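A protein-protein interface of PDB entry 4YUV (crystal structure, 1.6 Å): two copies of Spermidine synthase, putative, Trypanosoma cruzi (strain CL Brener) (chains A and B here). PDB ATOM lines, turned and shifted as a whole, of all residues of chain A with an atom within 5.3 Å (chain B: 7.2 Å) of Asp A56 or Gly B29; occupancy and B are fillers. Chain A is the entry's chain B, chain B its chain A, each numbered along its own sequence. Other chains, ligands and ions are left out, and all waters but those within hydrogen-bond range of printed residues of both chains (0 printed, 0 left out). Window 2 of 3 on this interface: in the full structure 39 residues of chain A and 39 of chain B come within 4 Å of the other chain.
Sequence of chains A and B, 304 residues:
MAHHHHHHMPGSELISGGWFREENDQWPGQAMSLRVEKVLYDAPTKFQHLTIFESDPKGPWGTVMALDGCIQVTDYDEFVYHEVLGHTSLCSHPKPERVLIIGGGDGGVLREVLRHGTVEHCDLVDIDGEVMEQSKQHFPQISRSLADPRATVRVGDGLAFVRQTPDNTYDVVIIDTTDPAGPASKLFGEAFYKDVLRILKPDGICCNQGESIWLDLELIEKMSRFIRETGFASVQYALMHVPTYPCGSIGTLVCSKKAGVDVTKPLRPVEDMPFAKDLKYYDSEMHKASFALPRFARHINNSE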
ATOM      1  N   TRP A  19     -12.516 -19.720  -5.208  1.00  0.00           N
ATOM      2  CA  TRP A  19     -13.275 -18.513  -5.036  1.00  0.00           C
ATOM      3  C   TRP A  19     -14.348 -18.343  -6.125  1.00  0.00           C
ATOM      4  O   TRP A  19     -14.172 -18.795  -7.269  1.00  0.00           O
ATOM      5  CB  TRP A  19     -12.321 -17.317  -5.099  1.00  0.00           C
ATOM      6  CG  TRP A  19     -11.363 -17.255  -3.901  1.00  0.00           C
ATOM      7  CD1 TRP A  19     -10.268 -18.072  -3.663  1.00  0.00           C
ATOM      8  CD2 TRP A  19     -11.420 -16.338  -2.797  1.00  0.00           C
ATOM      9  NE1 TRP A  19      -9.652 -17.713  -2.478  1.00  0.00           N
ATOM     10  CE2 TRP A  19     -10.323 -16.644  -1.934  1.00  0.00           C
ATOM     11  CE3 TRP A  19     -12.264 -15.268  -2.467  1.00  0.00           C
ATOM     12  CZ2 TRP A  19     -10.081 -15.938  -0.742  1.00  0.00           C
ATOM     13  CZ3 TRP A  19     -12.017 -14.552  -1.278  1.00  0.00           C
ATOM     14  CH2 TRP A  19     -10.931 -14.889  -0.442  1.00  0.00           C
ATOM     15  N   SER A  33     -15.278 -10.898  -4.393  1.00  0.00           N
ATOM     16  CA  SER A  33     -15.068 -12.322  -4.408  1.00  0.00           C
ATOM     17  C   SER A  33     -15.422 -12.858  -3.072  1.00  0.00           C
ATOM     18  O   SER A  33     -15.138 -12.258  -2.027  1.00  0.00           O
ATOM     19  CB  SER A  33     -13.581 -12.709  -4.675  1.00  0.00           C
ATOM     20  OG  SER A  33     -13.156 -12.141  -5.879  1.00  0.00           O
ATOM     21  N   LEU A  34     -15.983 -14.049  -3.093  1.00  0.00           N
ATOM     22  CA  LEU A  34     -16.221 -14.820  -1.895  1.00  0.00           C
ATOM     23  C   LEU A  34     -15.581 -16.135  -2.143  1.00  0.00           C
ATOM     24  O   LEU A  34     -15.641 -16.637  -3.280  1.00  0.00           O
ATOM     25  CB  LEU A  34     -17.717 -15.023  -1.666  1.00  0.00           C
ATOM     26  CG  LEU A  34     -18.471 -13.707  -1.320  1.00  0.00           C
ATOM     27  CD1 LEU A  34     -19.949 -13.728  -1.647  1.00  0.00           C
ATOM     28  CD2 LEU A  34     -18.237 -13.276   0.133  1.00  0.00           C
ATOM     29  N   ARG A  35     -15.023 -16.721  -1.107  1.00  0.00           N
ATOM     30  CA  ARG A  35     -14.374 -18.034  -1.230  1.00  0.00           C
ATOM     31  C   ARG A  35     -15.452 -19.145  -1.263  1.00  0.00           C
ATOM     32  O   ARG A  35     -16.468 -19.023  -0.620  1.00  0.00           O
ATOM     33  CB  ARG A  35     -13.445 -18.275  -0.029  1.00  0.00           C
ATOM     34  CG  ARG A  35     -12.585 -19.540  -0.181  1.00  0.00           C
ATOM     35  CD  ARG A  35     -11.643 -19.740   1.002  1.00  0.00           C
ATOM     36  NE  ARG A  35     -10.281 -20.097   0.609  1.00  0.00           N
ATOM     37  CZ  ARG A  35      -9.946 -21.242   0.017  1.00  0.00           C
ATOM     38  NH1 ARG A  35     -10.885 -22.142  -0.275  1.00  0.00           N
ATOM     39  NH2 ARG A  35      -8.675 -21.487  -0.293  1.00  0.00           N
ATOM     40  N   VAL A  36     -15.189 -20.276  -1.925  1.00  0.00           N
ATOM     41  CA  VAL A  36     -16.150 -21.394  -1.999  1.00  0.00           C
ATOM     42  C   VAL A  36     -15.774 -22.601  -1.164  1.00  0.00           C
ATOM     43  O   VAL A  36     -14.708 -23.221  -1.356  1.00  0.00           O
ATOM     44  CB  VAL A  36     -16.212 -21.835  -3.454  1.00  0.00           C
ATOM     45  CG1 VAL A  36     -17.137 -23.054  -3.673  1.00  0.00           C
ATOM     46  CG2 VAL A  36     -16.575 -20.643  -4.350  1.00  0.00           C
ATOM     47  N   GLU A  37     -16.587 -22.984  -0.217  1.00  0.00           N
ATOM     48  CA  GLU A  37     -16.308 -24.208   0.521  1.00  0.00           C
ATOM     49  C   GLU A  37     -16.821 -25.440  -0.278  1.00  0.00           C
ATOM     50  O   GLU A  37     -16.116 -26.466  -0.385  1.00  0.00           O
ATOM     51  CB  GLU A  37     -16.858 -24.138   1.946  1.00  0.00           C
ATOM     52  CG  GLU A  37     -16.651 -25.392   2.784  1.00  0.00           C
ATOM     53  CD  GLU A  37     -15.176 -25.727   3.022  1.00  0.00           C
ATOM     54  OE1 GLU A  37     -14.447 -24.946   3.687  1.00  0.00           O
ATOM     55  OE2 GLU A  37     -14.746 -26.796   2.565  1.00  0.00           O
ATOM     56  N   GLU A  54     -21.692 -22.844  -0.793  1.00  0.00           N
ATOM     57  CA  GLU A  54     -21.404 -22.623   0.613  1.00  0.00           C
ATOM     58  C   GLU A  54     -20.074 -21.868   0.641  1.00  0.00           C
ATOM     59  O   GLU A  54     -19.085 -22.280  -0.006  1.00  0.00           O
ATOM     60  CB  GLU A  54     -21.302 -23.964   1.413  1.00  0.00           C
ATOM     61  CG  GLU A  54     -21.327 -23.760   2.906  1.00  0.00           C
ATOM     62  CD  GLU A  54     -22.625 -23.058   3.381  1.00  0.00           C
ATOM     63  OE1 GLU A  54     -23.728 -23.467   2.926  1.00  0.00           O
ATOM     64  OE2 GLU A  54     -22.566 -22.090   4.191  1.00  0.00           O
ATOM     65  N   SER A  55     -20.069 -20.698   1.266  1.00  0.00           N
ATOM     66  CA  SER A  55     -18.844 -19.883   1.277  1.00  0.00           C
ATOM     67  C   SER A  55     -17.963 -20.394   2.417  1.00  0.00           C
ATOM     68  O   SER A  55     -18.325 -21.339   3.133  1.00  0.00           O
ATOM     69  CB  SER A  55     -19.237 -18.348   1.440  1.00  0.00           C
ATOM     70  OG  SER A  55     -19.812 -18.049   2.697  1.00  0.00           O
ATOM     71  N   ASP A  56     -16.818 -19.743   2.631  1.00  0.00           N
ATOM     72  CA  ASP A  56     -15.888 -20.147   3.736  1.00  0.00           C
ATOM     73  C   ASP A  56     -16.547 -20.219   5.130  1.00  0.00           C
ATOM     74  O   ASP A  56     -17.086 -19.225   5.555  1.00  0.00           O
ATOM     75  CB  ASP A  56     -14.757 -19.122   3.764  1.00  0.00           C
ATOM     76  CG  ASP A  56     -13.575 -19.580   4.573  1.00  0.00           C
ATOM     77  OD1 ASP A  56     -13.732 -20.458   5.456  1.00  0.00           O
ATOM     78  OD2 ASP A  56     -12.504 -18.992   4.325  1.00  0.00           O
ATOM     79  N   PRO A  57     -16.554 -21.419   5.824  1.00  0.00           N
ATOM     80  CA  PRO A  57     -17.235 -21.466   7.148  1.00  0.00           C
ATOM     81  C   PRO A  57     -16.474 -20.694   8.199  1.00  0.00           C
ATOM     82  O   PRO A  57     -16.985 -20.415   9.295  1.00  0.00           O
ATOM     83  CB  PRO A  57     -17.291 -22.972   7.494  1.00  0.00           C
ATOM     84  CG  PRO A  57     -16.215 -23.589   6.661  1.00  0.00           C
ATOM     85  CD  PRO A  57     -16.091 -22.765   5.414  1.00  0.00           C
ATOM     86  N   LYS A  58     -15.259 -20.298   7.840  1.00  0.00           N
ATOM     87  CA  LYS A  58     -14.459 -19.451   8.676  1.00  0.00           C
ATOM     88  C   LYS A  58     -14.953 -18.013   8.580  1.00  0.00           C
ATOM     89  O   LYS A  58     -14.702 -17.211   9.474  1.00  0.00           O
ATOM     90  CB  LYS A  58     -12.982 -19.555   8.255  1.00  0.00           C
ATOM     91  CG  LYS A  58     -12.006 -19.222   9.382  1.00  0.00           C
ATOM     92  CD  LYS A  58     -10.914 -18.247   8.894  1.00  0.00           C
ATOM     93  CE  LYS A  58      -9.548 -18.914   8.650  1.00  0.00           C
ATOM     94  NZ  LYS A  58      -9.090 -19.711   9.840  1.00  0.00           N
ATOM     95  N   GLY A  59     -15.670 -17.696   7.489  1.00  0.00           N
ATOM     96  CA  GLY A  59     -16.313 -16.388   7.367  1.00  0.00           C
ATOM     97  C   GLY A  59     -17.802 -16.386   7.750  1.00  0.00           C
ATOM     98  O   GLY A  59     -18.366 -17.420   8.062  1.00  0.00           O
ATOM     99  N   PRO A  60     -18.448 -15.212   7.671  1.00  0.00           N
ATOM    100  CA  PRO A  60     -19.819 -15.099   8.119  1.00  0.00           C
ATOM    101  C   PRO A  60     -20.871 -15.298   7.008  1.00  0.00           C
ATOM    102  O   PRO A  60     -22.036 -15.306   7.329  1.00  0.00           O
ATOM    103  CB  PRO A  60     -19.872 -13.640   8.599  1.00  0.00           C
ATOM    104  CG  PRO A  60     -19.028 -12.917   7.567  1.00  0.00           C
ATOM    105  CD  PRO A  60     -17.850 -13.877   7.419  1.00  0.00           C
ATOM    106  N   TRP A  61     -20.458 -15.416   5.740  1.00  0.00           N
ATOM    107  CA  TRP A  61     -21.426 -15.198   4.629  1.00  0.00           C
ATOM    108  C   TRP A  61     -22.455 -16.286   4.454  1.00  0.00           C
ATOM    109  O   TRP A  61     -23.540 -16.017   3.918  1.00  0.00           O
ATOM    110  CB  TRP A  61     -20.774 -14.800   3.309  1.00  0.00           C
ATOM    111  CG  TRP A  61     -19.967 -13.613   3.592  1.00  0.00           C
ATOM    112  CD1 TRP A  61     -18.629 -13.596   3.824  1.00  0.00           C
ATOM    113  CD2 TRP A  61     -20.437 -12.244   3.747  1.00  0.00           C
ATOM    114  NE1 TRP A  61     -18.214 -12.303   4.114  1.00  0.00           N
ATOM    115  CE2 TRP A  61     -19.311 -11.465   4.050  1.00  0.00           C
ATOM    116  CE3 TRP A  61     -21.719 -11.609   3.673  1.00  0.00           C
ATOM    117  CZ2 TRP A  61     -19.376 -10.074   4.297  1.00  0.00           C
ATOM    118  CZ3 TRP A  61     -21.781 -10.145   3.884  1.00  0.00           C
ATOM    119  CH2 TRP A  61     -20.609  -9.436   4.201  1.00  0.00           C
ATOM    120  N   GLU B  23      -7.500  -8.847   0.611  1.00  0.00           N
ATOM    121  CA  GLU B  23      -8.006  -9.807   1.602  1.00  0.00           C
ATOM    122  C   GLU B  23      -7.131  -9.748   2.871  1.00  0.00           C
ATOM    123  O   GLU B  23      -5.911  -9.507   2.780  1.00  0.00           O
ATOM    124  CB  GLU B  23      -8.130 -11.243   1.041  1.00  0.00           C
ATOM    125  CG  GLU B  23      -6.879 -11.873   0.434  1.00  0.00           C
ATOM    126  CD  GLU B  23      -7.102 -13.312  -0.044  1.00  0.00           C
ATOM    127  OE1 GLU B  23      -7.586 -14.139   0.770  1.00  0.00           O
ATOM    128  OE2 GLU B  23      -6.784 -13.621  -1.224  1.00  0.00           O
ATOM    129  N   ASN B  24      -7.784  -9.883   4.037  1.00  0.00           N
ATOM    130  CA  ASN B  24      -7.126  -9.886   5.349  1.00  0.00           C
ATOM    131  C   ASN B  24      -7.630 -11.036   6.242  1.00  0.00           C
ATOM    132  O   ASN B  24      -8.845 -11.302   6.330  1.00  0.00           O
ATOM    133  CB  ASN B  24      -7.291  -8.517   6.046  1.00  0.00           C
ATOM    134  CG  ASN B  24      -6.334  -7.444   5.499  1.00  0.00           C
ATOM    135  OD1 ASN B  24      -5.488  -6.908   6.233  1.00  0.00           O
ATOM    136  ND2 ASN B  24      -6.463  -7.126   4.212  1.00  0.00           N
ATOM    137  N   PRO B  28     -12.618 -12.424   6.466  1.00  0.00           N
ATOM    138  CA  PRO B  28     -12.323 -13.831   6.194  1.00  0.00           C
ATOM    139  C   PRO B  28     -13.210 -14.528   5.126  1.00  0.00           C
ATOM    140  O   PRO B  28     -14.407 -14.749   5.313  1.00  0.00           O
ATOM    141  CB  PRO B  28     -12.433 -14.460   7.588  1.00  0.00           C
ATOM    142  CG  PRO B  28     -11.953 -13.344   8.504  1.00  0.00           C
ATOM    143  CD  PRO B  28     -12.035 -12.022   7.762  1.00  0.00           C
ATOM    144  N   GLY B  29     -12.606 -14.889   4.001  1.00  0.00           N
ATOM    145  CA  GLY B  29     -13.361 -15.540   2.947  1.00  0.00           C
ATOM    146  C   GLY B  29     -14.046 -14.522   2.056  1.00  0.00           C
ATOM    147  O   GLY B  29     -15.024 -14.809   1.375  1.00  0.00           O
ATOM    148  N   GLN B  30     -13.526 -13.304   2.065  1.00  0.00           N
ATOM    149  CA  GLN B  30     -14.025 -12.304   1.173  1.00  0.00           C
ATOM    150  C   GLN B  30     -12.817 -11.495   0.699  1.00  0.00           C
ATOM    151  O   GLN B  30     -11.792 -11.402   1.398  1.00  0.00           O
ATOM    152  CB  GLN B  30     -15.050 -11.400   1.881  1.00  0.00           C
ATOM    153  CG  GLN B  30     -14.360 -10.338   2.752  1.00  0.00           C
ATOM    154  CD  GLN B  30     -15.294  -9.513   3.635  1.00  0.00           C
ATOM    155  OE1 GLN B  30     -15.221  -8.283   3.646  1.00  0.00           O
ATOM    156  NE2 GLN B  30     -16.120 -10.190   4.429  1.00  0.00           N
ATOM    157  N   ALA B  31     -12.942 -10.914  -0.485  1.00  0.00           N
ATOM    158  CA  ALA B  31     -11.924  -9.988  -0.988  1.00  0.00           C
ATOM    159  C   ALA B  31     -12.586  -9.022  -1.936  1.00  0.00           C
ATOM    160  O   ALA B  31     -13.520  -9.362  -2.688  1.00  0.00           O
ATOM    161  CB  ALA B  31     -10.820 -10.775  -1.684  1.00  0.00           C
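Of the printed residues of chain B, Leu A34 touches Gly B29. Of chain B, only Gly B29 (3.8 Å) comes within 4 Å of Asp A56. Printed residues of chain A within 4 Å of Glu B23: Trp A19. Gly B29 touches four residues of chain A. The nearest residue of chain A that does not touch Gly B29 is Ser A33 (4.3 Å).
The backbone carbonyl oxygen (O) of Arg A35 lies within hydrogen-bond range of the backbone NH (N) of Asp A56, at 3.3 Å. N of Lys A58 is in hydrogen-bond range of OD1 of Asp A56 (2.8 Å).
No position is printed for both chains. Of the 11 pairs that touch across the chains among the printed residues, none has its exchanged pair printed and touching as well.
The backbone carbonyl oxygen of Gly B29 is in hydrogen-bond range of the backbone NH of Arg A35, 3.1 Å away. NE1 of Trp A61 lies close to NE2 of Gln B30 (3.0 Å). The backbone carbonyl oxygen (O) of Ala B31 lies within hydrogen-bond range of the backbone NH (N) of Ser A33 (2.9 Å).
Hydrophobic or aromatic side chains of chain A that line the printed part of chain B: Trp A19, Leu A34 and Trp A61. Printed residues of chain B that touch a printed residue of chain A: Glu B23, Pro B28, Gly B29, Gln B30 and Ala B31. Hydrophobic or aromatic side chains of chain B within 4 Å of the printed part of chain A: Ala B31.
Among the printed residues, pairs that only touch across the chains: Gly A59 with Pro B28, Ser A33 with Gln B30, Trp A19 with Glu B23, Leu A34 with Gly B29, Trp A19 with Gln B30, Asp A56 with Gly B29, Trp A19 with Ala B31 and Trp A19 with Gly B29.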
